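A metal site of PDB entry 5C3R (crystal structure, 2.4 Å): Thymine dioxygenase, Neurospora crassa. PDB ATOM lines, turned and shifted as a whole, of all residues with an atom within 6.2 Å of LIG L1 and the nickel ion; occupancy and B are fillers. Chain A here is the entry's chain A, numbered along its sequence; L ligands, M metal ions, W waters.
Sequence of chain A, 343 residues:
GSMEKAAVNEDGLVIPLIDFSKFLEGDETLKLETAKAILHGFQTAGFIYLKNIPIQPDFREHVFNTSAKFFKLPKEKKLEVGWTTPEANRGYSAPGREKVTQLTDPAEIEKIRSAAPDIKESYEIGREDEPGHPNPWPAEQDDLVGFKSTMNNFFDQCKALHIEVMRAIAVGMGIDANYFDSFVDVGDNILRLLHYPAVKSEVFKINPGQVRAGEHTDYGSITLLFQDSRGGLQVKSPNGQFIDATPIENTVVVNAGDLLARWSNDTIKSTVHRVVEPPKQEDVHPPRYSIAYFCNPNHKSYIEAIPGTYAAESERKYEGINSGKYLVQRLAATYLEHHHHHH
The side-chain hydroxyl of Tyr 196 is in hydrogen-bond range of an oxygen (O5) of LIG L1, at 2.7 Å.
OG of Ser 290 sits at hydrogen-bond distance from O5 of LIG L1 (2.7 Å).
NH2 of Arg 288 is in salt-bridge range of O4 of LIG L1 (2.7 Å).
The guanidinium group of Arg 192 lies within salt-bridge range of an oxygen (O2) of LIG L1, 2.9 Å away.
O2 of LG2 L2 sits close to O1 of LIG L1, 2.6 Å away.
OD2 of Asp 218 sits at hydrogen-bond distance from ND2 of Asn 255 (3.1 Å).
OD2 of Asp 218 is in hydrogen-bond range of OG1 of Thr 223 (2.7 Å).
O of Arg 288 is in hydrogen-bond range of N of Tyr 196 (2.7 Å).
The backbone carbonyl oxygen (O) of Ser 290 lies within hydrogen-bond range of the backbone NH (N) of Leu 194 (3.0 Å).
The guanidinium group of Arg 288 is in hydrogen-bond range of the side-chain amide oxygen of Gln 227, at 3.2 Å.
The backbone NH of Arg 192 is in hydrogen-bond range of the backbone carbonyl oxygen of Ala 292.
The backbone carbonyl oxygen (O) of Val 275 sits at hydrogen-bond distance from the backbone NH (N) of Ala 213 (2.9 Å).
Merely in contact with LIG L1: Leu 194 (3.6 Å), Leu 225 (3.5 Å), Leu 233 (3.99 Å), Val 275 (3.5 Å) and Phe 294 (3.4 Å).
Hydrophobic or aromatic side chains within 4 Å of LIG L1: Leu 194, Tyr 196, His 216, Leu 225, Leu 233, His 273, Val 275 and Phe 294.
Within 4 Å of LIG L1: Arg 192, Leu 194, Tyr 196, His 216, Asp 218, Leu 225, Leu 233, His 273, Val 275, Arg 288, Ser 290 and Phe 294.
The nearest printed residue that does not touch LIG L1 is Ala 292 (4.02 Å).
Of the 22 residues printed, 3 come within 4 Å of the nickel ion.
An oxygen (O3) of LIG L1 is bound to the nickel ion (2.1 Å).
O1 of LIG L1 is bound to the nickel ion (2.2 Å).
OD1 of Asp 218 binds the nickel ion, 2.2 Å away.
The nickel ion is bound by water W1, at 2.3 Å.
The nickel ion is bound by NE2 of His 216 (2.3 Å).
The nickel ion is bound by NE2 of His 273.
The nickel ion has six donor atoms within binding distance.
Water W2 lies within hydrogen-bond range of OH of Tyr 196 and O2 of LIG L1.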
ATOM      1  N   LYS A 120      -0.661   0.285 -22.516  1.00  0.00           N
ATOM      2  CA  LYS A 120      -1.518  -0.663 -21.817  1.00  0.00           C
ATOM      3  C   LYS A 120      -1.857  -1.851 -22.696  1.00  0.00           C
ATOM      4  O   LYS A 120      -1.653  -1.826 -23.909  1.00  0.00           O
ATOM      5  CB  LYS A 120      -2.809   0.028 -21.350  1.00  0.00           C
ATOM      6  CG  LYS A 120      -3.781   0.406 -22.472  1.00  0.00           C
ATOM      7  CD  LYS A 120      -4.909   1.303 -21.962  1.00  0.00           C
ATOM      8  CE  LYS A 120      -5.976   1.525 -23.024  1.00  0.00           C
ATOM      9  NZ  LYS A 120      -6.987   0.423 -23.039  1.00  0.00           N
ATOM     10  N   ARG A 192     -13.005  -6.208 -17.557  1.00  0.00           N
ATOM     11  CA  ARG A 192     -11.801  -5.806 -18.259  1.00  0.00           C
ATOM     12  C   ARG A 192     -10.573  -5.957 -17.363  1.00  0.00           C
ATOM     13  O   ARG A 192     -10.398  -5.211 -16.408  1.00  0.00           O
ATOM     14  CB  ARG A 192     -11.921  -4.356 -18.740  1.00  0.00           C
ATOM     15  CG  ARG A 192     -10.669  -3.828 -19.450  1.00  0.00           C
ATOM     16  CD  ARG A 192     -10.750  -2.355 -19.785  1.00  0.00           C
ATOM     17  NE  ARG A 192     -11.215  -2.099 -21.151  1.00  0.00           N
ATOM     18  CZ  ARG A 192     -11.285  -0.892 -21.724  1.00  0.00           C
ATOM     19  NH1 ARG A 192     -10.950   0.210 -21.041  1.00  0.00           N
ATOM     20  NH2 ARG A 192     -11.707  -0.778 -22.970  1.00  0.00           N
ATOM     21  N   LEU A 194      -6.661  -5.415 -16.932  1.00  0.00           N
ATOM     22  CA  LEU A 194      -5.743  -4.416 -17.462  1.00  0.00           C
ATOM     23  C   LEU A 194      -4.333  -4.638 -16.945  1.00  0.00           C
ATOM     24  O   LEU A 194      -4.131  -4.945 -15.774  1.00  0.00           O
ATOM     25  CB  LEU A 194      -6.197  -3.000 -17.079  1.00  0.00           C
ATOM     26  CG  LEU A 194      -7.310  -2.388 -17.927  1.00  0.00           C
ATOM     27  CD1 LEU A 194      -8.109  -1.367 -17.119  1.00  0.00           C
ATOM     28  CD2 LEU A 194      -6.722  -1.749 -19.170  1.00  0.00           C
ATOM     29  N   TYR A 196      -0.701  -2.475 -17.348  1.00  0.00           N
ATOM     30  CA  TYR A 196       0.083  -1.342 -17.817  1.00  0.00           C
ATOM     31  C   TYR A 196       1.543  -1.704 -17.569  1.00  0.00           C
ATOM     32  O   TYR A 196       1.999  -1.653 -16.422  1.00  0.00           O
ATOM     33  CB  TYR A 196      -0.288  -0.066 -17.047  1.00  0.00           C
ATOM     34  CG  TYR A 196      -1.756   0.329 -17.112  1.00  0.00           C
ATOM     35  CD1 TYR A 196      -2.214   1.206 -18.091  1.00  0.00           C
ATOM     36  CD2 TYR A 196      -2.674  -0.138 -16.187  1.00  0.00           C
ATOM     37  CE1 TYR A 196      -3.548   1.579 -18.157  1.00  0.00           C
ATOM     38  CE2 TYR A 196      -4.019   0.221 -16.250  1.00  0.00           C
ATOM     39  CZ  TYR A 196      -4.442   1.084 -17.235  1.00  0.00           C
ATOM     40  OH  TYR A 196      -5.757   1.466 -17.295  1.00  0.00           O
ATOM     41  N   ALA A 213      -3.622   5.538 -19.640  1.00  0.00           N
ATOM     42  CA  ALA A 213      -4.982   5.432 -20.176  1.00  0.00           C
ATOM     43  C   ALA A 213      -5.549   6.825 -20.434  1.00  0.00           C
ATOM     44  O   ALA A 213      -5.547   7.660 -19.534  1.00  0.00           O
ATOM     45  CB  ALA A 213      -5.891   4.670 -19.238  1.00  0.00           C
ATOM     46  N   HIS A 216     -11.450   9.862 -20.350  1.00  0.00           N
ATOM     47  CA  HIS A 216     -12.713   9.399 -20.880  1.00  0.00           C
ATOM     48  C   HIS A 216     -13.747   9.375 -19.774  1.00  0.00           C
ATOM     49  O   HIS A 216     -13.419   9.560 -18.603  1.00  0.00           O
ATOM     50  CB  HIS A 216     -12.552   7.981 -21.420  1.00  0.00           C
ATOM     51  CG  HIS A 216     -12.127   7.002 -20.387  1.00  0.00           C
ATOM     52  ND1 HIS A 216     -10.826   6.928 -19.916  1.00  0.00           N
ATOM     53  CD2 HIS A 216     -12.820   6.077 -19.687  1.00  0.00           C
ATOM     54  CE1 HIS A 216     -10.741   5.979 -19.002  1.00  0.00           C
ATOM     55  NE2 HIS A 216     -11.941   5.451 -18.843  1.00  0.00           N
ATOM     56  N   THR A 217     -14.990   9.169 -20.180  1.00  0.00           N
ATOM     57  CA  THR A 217     -16.047   8.759 -19.273  1.00  0.00           C
ATOM     58  C   THR A 217     -16.384   7.324 -19.617  1.00  0.00           C
ATOM     59  O   THR A 217     -16.291   6.925 -20.785  1.00  0.00           O
ATOM     60  CB  THR A 217     -17.295   9.650 -19.442  1.00  0.00           C
ATOM     61  OG1 THR A 217     -17.707   9.660 -20.824  1.00  0.00           O
ATOM     62  CG2 THR A 217     -17.001  11.063 -18.998  1.00  0.00           C
ATOM     63  N   ASP A 218     -16.760   6.532 -18.615  1.00  0.00           N
ATOM     64  CA  ASP A 218     -17.296   5.183 -18.851  1.00  0.00           C
ATOM     65  C   ASP A 218     -18.717   5.283 -19.380  1.00  0.00           C
ATOM     66  O   ASP A 218     -19.392   6.303 -19.191  1.00  0.00           O
ATOM     67  CB  ASP A 218     -17.280   4.348 -17.570  1.00  0.00           C
ATOM     68  CG  ASP A 218     -15.869   4.100 -17.036  1.00  0.00           C
ATOM     69  OD1 ASP A 218     -14.878   4.427 -17.747  1.00  0.00           O
ATOM     70  OD2 ASP A 218     -15.762   3.587 -15.909  1.00  0.00           O
ATOM     71  N   THR A 223     -19.032   1.314 -12.772  1.00  0.00           N
ATOM     72  CA  THR A 223     -17.815   0.567 -12.994  1.00  0.00           C
ATOM     73  C   THR A 223     -17.196   0.271 -11.636  1.00  0.00           C
ATOM     74  O   THR A 223     -17.008   1.172 -10.816  1.00  0.00           O
ATOM     75  CB  THR A 223     -16.821   1.366 -13.853  1.00  0.00           C
ATOM     76  OG1 THR A 223     -17.390   1.582 -15.142  1.00  0.00           O
ATOM     77  CG2 THR A 223     -15.500   0.620 -14.020  1.00  0.00           C
ATOM     78  N   LEU A 225     -13.911  -0.556 -10.046  1.00  0.00           N
ATOM     79  CA  LEU A 225     -12.499  -0.489 -10.371  1.00  0.00           C
ATOM     80  C   LEU A 225     -11.640  -0.930  -9.194  1.00  0.00           C
ATOM     81  O   LEU A 225     -11.597  -0.277  -8.160  1.00  0.00           O
ATOM     82  CB  LEU A 225     -12.118   0.934 -10.808  1.00  0.00           C
ATOM     83  CG  LEU A 225     -10.688   1.098 -11.307  1.00  0.00           C
ATOM     84  CD1 LEU A 225     -10.397   0.260 -12.537  1.00  0.00           C
ATOM     85  CD2 LEU A 225     -10.421   2.558 -11.603  1.00  0.00           C
ATOM     86  N   PHE A 226     -10.964  -2.066  -9.396  1.00  0.00           N
ATOM     87  CA  PHE A 226     -10.029  -2.634  -8.447  1.00  0.00           C
ATOM     88  C   PHE A 226      -8.618  -2.260  -8.937  1.00  0.00           C
ATOM     89  O   PHE A 226      -8.208  -2.707 -10.012  1.00  0.00           O
ATOM     90  CB  PHE A 226     -10.175  -4.154  -8.418  1.00  0.00           C
ATOM     91  CG  PHE A 226     -11.574  -4.641  -8.120  1.00  0.00           C
ATOM     92  CD1 PHE A 226     -12.534  -4.714  -9.108  1.00  0.00           C
ATOM     93  CD2 PHE A 226     -11.907  -5.056  -6.839  1.00  0.00           C
ATOM     94  CE1 PHE A 226     -13.806  -5.179  -8.835  1.00  0.00           C
ATOM     95  CE2 PHE A 226     -13.194  -5.521  -6.552  1.00  0.00           C
ATOM     96  CZ  PHE A 226     -14.143  -5.584  -7.557  1.00  0.00           C
ATOM     97  N   GLN A 227      -7.901  -1.447  -8.176  1.00  0.00           N
ATOM     98  CA  GLN A 227      -6.534  -1.050  -8.567  1.00  0.00           C
ATOM     99  C   GLN A 227      -5.507  -1.555  -7.562  1.00  0.00           C
ATOM    100  O   GLN A 227      -5.797  -1.724  -6.383  1.00  0.00           O
ATOM    101  CB  GLN A 227      -6.417   0.465  -8.731  1.00  0.00           C
ATOM    102  CG  GLN A 227      -6.701   1.280  -7.478  1.00  0.00           C
ATOM    103  CD  GLN A 227      -6.409   2.759  -7.657  1.00  0.00           C
ATOM    104  OE1 GLN A 227      -5.645   3.155  -8.543  1.00  0.00           O
ATOM    105  NE2 GLN A 227      -7.021   3.579  -6.806  1.00  0.00           N
ATOM    106  N   LEU A 233      -4.208   6.685 -11.365  1.00  0.00           N
ATOM    107  CA  LEU A 233      -5.597   7.033 -11.654  1.00  0.00           C
ATOM    108  C   LEU A 233      -5.884   8.446 -11.162  1.00  0.00           C
ATOM    109  O   LEU A 233      -5.544   8.796 -10.039  1.00  0.00           O
ATOM    110  CB  LEU A 233      -6.560   6.040 -11.010  1.00  0.00           C
ATOM    111  CG  LEU A 233      -8.054   6.332 -11.118  1.00  0.00           C
ATOM    112  CD1 LEU A 233      -8.537   6.283 -12.561  1.00  0.00           C
ATOM    113  CD2 LEU A 233      -8.853   5.349 -10.266  1.00  0.00           C
ATOM    114  N   ASN A 255     -17.519   4.167  -9.855  1.00  0.00           N
ATOM    115  CA  ASN A 255     -17.941   5.373 -10.530  1.00  0.00           C
ATOM    116  C   ASN A 255     -19.137   5.140 -11.433  1.00  0.00           C
ATOM    117  O   ASN A 255     -19.295   4.070 -12.012  1.00  0.00           O
ATOM    118  CB  ASN A 255     -16.785   5.981 -11.329  1.00  0.00           C
ATOM    119  CG  ASN A 255     -16.332   5.091 -12.458  1.00  0.00           C
ATOM    120  OD1 ASN A 255     -15.675   4.074 -12.237  1.00  0.00           O
ATOM    121  ND2 ASN A 255     -16.654   5.482 -13.684  1.00  0.00           N
ATOM    122  N   HIS A 273     -12.051  10.688 -16.142  1.00  0.00           N
ATOM    123  CA  HIS A 273     -10.882  10.146 -15.455  1.00  0.00           C
ATOM    124  C   HIS A 273      -9.863   9.598 -16.457  1.00  0.00           C
ATOM    125  O   HIS A 273     -10.137   9.493 -17.643  1.00  0.00           O
ATOM    126  CB  HIS A 273     -11.309   9.085 -14.434  1.00  0.00           C
ATOM    127  CG  HIS A 273     -12.173   8.010 -15.014  1.00  0.00           C
ATOM    128  ND1 HIS A 273     -13.467   8.246 -15.420  1.00  0.00           N
ATOM    129  CD2 HIS A 273     -11.925   6.702 -15.253  1.00  0.00           C
ATOM    130  CE1 HIS A 273     -13.972   7.127 -15.905  1.00  0.00           C
ATOM    131  NE2 HIS A 273     -13.057   6.181 -15.818  1.00  0.00           N
ATOM    132  N   ARG A 274      -8.679   9.268 -15.962  1.00  0.00           N
ATOM    133  CA  ARG A 274      -7.563   8.838 -16.799  1.00  0.00           C
ATOM    134  C   ARG A 274      -6.521   8.149 -15.939  1.00  0.00           C
ATOM    135  O   ARG A 274      -6.633   8.160 -14.714  1.00  0.00           O
ATOM    136  CB  ARG A 274      -6.940  10.041 -17.504  1.00  0.00           C
ATOM    137  CG  ARG A 274      -6.336  11.065 -16.556  1.00  0.00           C
ATOM    138  CD  ARG A 274      -5.679  12.209 -17.298  1.00  0.00           C
ATOM    139  NE  ARG A 274      -4.805  12.978 -16.408  1.00  0.00           N
ATOM    140  CZ  ARG A 274      -4.115  14.063 -16.773  1.00  0.00           C
ATOM    141  NH1 ARG A 274      -4.205  14.544 -17.999  1.00  0.00           N
ATOM    142  NH2 ARG A 274      -3.340  14.662 -15.887  1.00  0.00           N
ATOM    143  N   VAL A 275      -5.508   7.569 -16.577  1.00  0.00           N
ATOM    144  CA  VAL A 275      -4.361   7.026 -15.870  1.00  0.00           C
ATOM    145  C   VAL A 275      -3.065   7.605 -16.428  1.00  0.00           C
ATOM    146  O   VAL A 275      -2.740   7.408 -17.597  1.00  0.00           O
ATOM    147  CB  VAL A 275      -4.317   5.487 -15.944  1.00  0.00           C
ATOM    148  CG1 VAL A 275      -3.194   4.960 -15.057  1.00  0.00           C
ATOM    149  CG2 VAL A 275      -5.649   4.899 -15.499  1.00  0.00           C
ATOM    150  N   ARG A 288       1.713  -1.854 -13.640  1.00  0.00           N
ATOM    151  CA  ARG A 288       0.480  -1.546 -12.930  1.00  0.00           C
ATOM    152  C   ARG A 288      -0.636  -2.468 -13.415  1.00  0.00           C
ATOM    153  O   ARG A 288      -0.858  -2.618 -14.618  1.00  0.00           O
ATOM    154  CB  ARG A 288       0.075  -0.081 -13.144  1.00  0.00           C
ATOM    155  CG  ARG A 288      -1.255   0.289 -12.511  1.00  0.00           C
ATOM    156  CD  ARG A 288      -1.482   1.791 -12.487  1.00  0.00           C
ATOM    157  NE  ARG A 288      -2.712   2.135 -11.775  1.00  0.00           N
ATOM    158  CZ  ARG A 288      -3.933   2.124 -12.306  1.00  0.00           C
ATOM    159  NH1 ARG A 288      -4.124   1.791 -13.578  1.00  0.00           N
ATOM    160  NH2 ARG A 288      -4.990   2.442 -11.553  1.00  0.00           N
ATOM    161  N   SER A 290      -4.788  -3.321 -12.936  1.00  0.00           N
ATOM    162  CA  SER A 290      -6.094  -2.961 -12.440  1.00  0.00           C
ATOM    163  C   SER A 290      -7.124  -3.858 -13.113  1.00  0.00           C
ATOM    164  O   SER A 290      -6.810  -4.528 -14.098  1.00  0.00           O
ATOM    165  CB  SER A 290      -6.404  -1.492 -12.698  1.00  0.00           C
ATOM    166  OG  SER A 290      -6.538  -1.222 -14.089  1.00  0.00           O
ATOM    167  N   ILE A 291      -8.334  -3.873 -12.567  1.00  0.00           N
ATOM    168  CA  ILE A 291      -9.451  -4.596 -13.144  1.00  0.00           C
ATOM    169  C   ILE A 291     -10.665  -3.685 -13.144  1.00  0.00           C
ATOM    170  O   ILE A 291     -11.131  -3.248 -12.071  1.00  0.00           O
ATOM    171  CB  ILE A 291      -9.771  -5.873 -12.346  1.00  0.00           C
ATOM    172  CG1 ILE A 291      -8.565  -6.824 -12.356  1.00  0.00           C
ATOM    173  CG2 ILE A 291     -11.004  -6.560 -12.932  1.00  0.00           C
ATOM    174  CD1 ILE A 291      -8.786  -8.110 -11.582  1.00  0.00           C
ATOM    175  N   ALA A 292     -11.194  -3.410 -14.343  1.00  0.00           N
ATOM    176  CA  ALA A 292     -12.392  -2.599 -14.501  1.00  0.00           C
ATOM    177  C   ALA A 292     -13.550  -3.503 -14.869  1.00  0.00           C
ATOM    178  O   ALA A 292     -13.577  -4.071 -15.961  1.00  0.00           O
ATOM    179  CB  ALA A 292     -12.182  -1.539 -15.567  1.00  0.00           C
ATOM    180  N   PHE A 294     -17.053  -3.290 -15.925  1.00  0.00           N
ATOM    181  CA  PHE A 294     -18.054  -2.374 -16.430  1.00  0.00           C
ATOM    182  C   PHE A 294     -19.434  -2.988 -16.244  1.00  0.00           C
ATOM    183  O   PHE A 294     -19.721  -4.048 -16.802  1.00  0.00           O
ATOM    184  CB  PHE A 294     -17.804  -2.073 -17.906  1.00  0.00           C
ATOM    185  CG  PHE A 294     -16.459  -1.470 -18.174  1.00  0.00           C
ATOM    186  CD1 PHE A 294     -16.100  -0.266 -17.599  1.00  0.00           C
ATOM    187  CD2 PHE A 294     -15.544  -2.101 -19.007  1.00  0.00           C
ATOM    188  CE1 PHE A 294     -14.862   0.302 -17.836  1.00  0.00           C
ATOM    189  CE2 PHE A 294     -14.312  -1.538 -19.251  1.00  0.00           C
ATOM    190  CZ  PHE A 294     -13.961  -0.334 -18.668  1.00  0.00           C
HETATM  191  C1  LIG L   1     -11.099   2.071 -17.828  1.00  0.00           C
HETATM  192  O1  LIG L   1     -12.180   2.517 -18.255  1.00  0.00           O
HETATM  193  O2  LIG L   1     -10.621   1.003 -18.261  1.00  0.00           O
HETATM  194  C2  LIG L   1     -10.376   2.832 -16.793  1.00  0.00           C
HETATM  195  O3  LIG L   1     -10.822   3.912 -16.413  1.00  0.00           O
HETATM  196  C3  LIG L   1      -9.070   2.275 -16.238  1.00  0.00           C
HETATM  197  C4  LIG L   1      -8.670   2.944 -14.918  1.00  0.00           C
HETATM  198  C5  LIG L   1      -7.523   2.223 -14.240  1.00  0.00           C
HETATM  199  O4  LIG L   1      -7.279   2.528 -13.058  1.00  0.00           O
HETATM  200  O5  LIG L   1      -6.840   1.360 -14.851  1.00  0.00           O
HETATM  201  N1  LG2 L   2     -15.415  -0.373 -22.474  1.00  0.00           N
HETATM  202  C1  LG2 L   2     -16.732  -0.692 -21.925  1.00  0.00           C
HETATM  203  O1  LG2 L   2     -17.284  -1.729 -22.209  1.00  0.00           O
HETATM  204  N2  LG2 L   2     -17.384   0.271 -21.015  1.00  0.00           N
HETATM  205  C2  LG2 L   2     -16.720   1.487 -20.683  1.00  0.00           C
HETATM  206  O2  LG2 L   2     -13.307   2.768 -20.640  1.00  0.00           O
HETATM  207  O3  LG2 L   2     -17.265   2.257 -19.936  1.00  0.00           O
HETATM  208  C3  LG2 L   2     -15.396   1.784 -21.239  1.00  0.00           C
HETATM  209  C4  LG2 L   2     -14.665   3.067 -20.909  1.00  0.00           C
HETATM  210  C5  LG2 L   2     -14.761   0.830 -22.139  1.00  0.00           C
HETATM  211 NI    NI M   1     -12.774   4.257 -17.065  1.00  0.00          NI
HETATM  212  O   HOH W   1     -13.341   3.001 -15.277  1.00  0.00           O
HETATM  213  O   HOH W   2      -7.908   1.495 -19.316  1.00  0.00           O
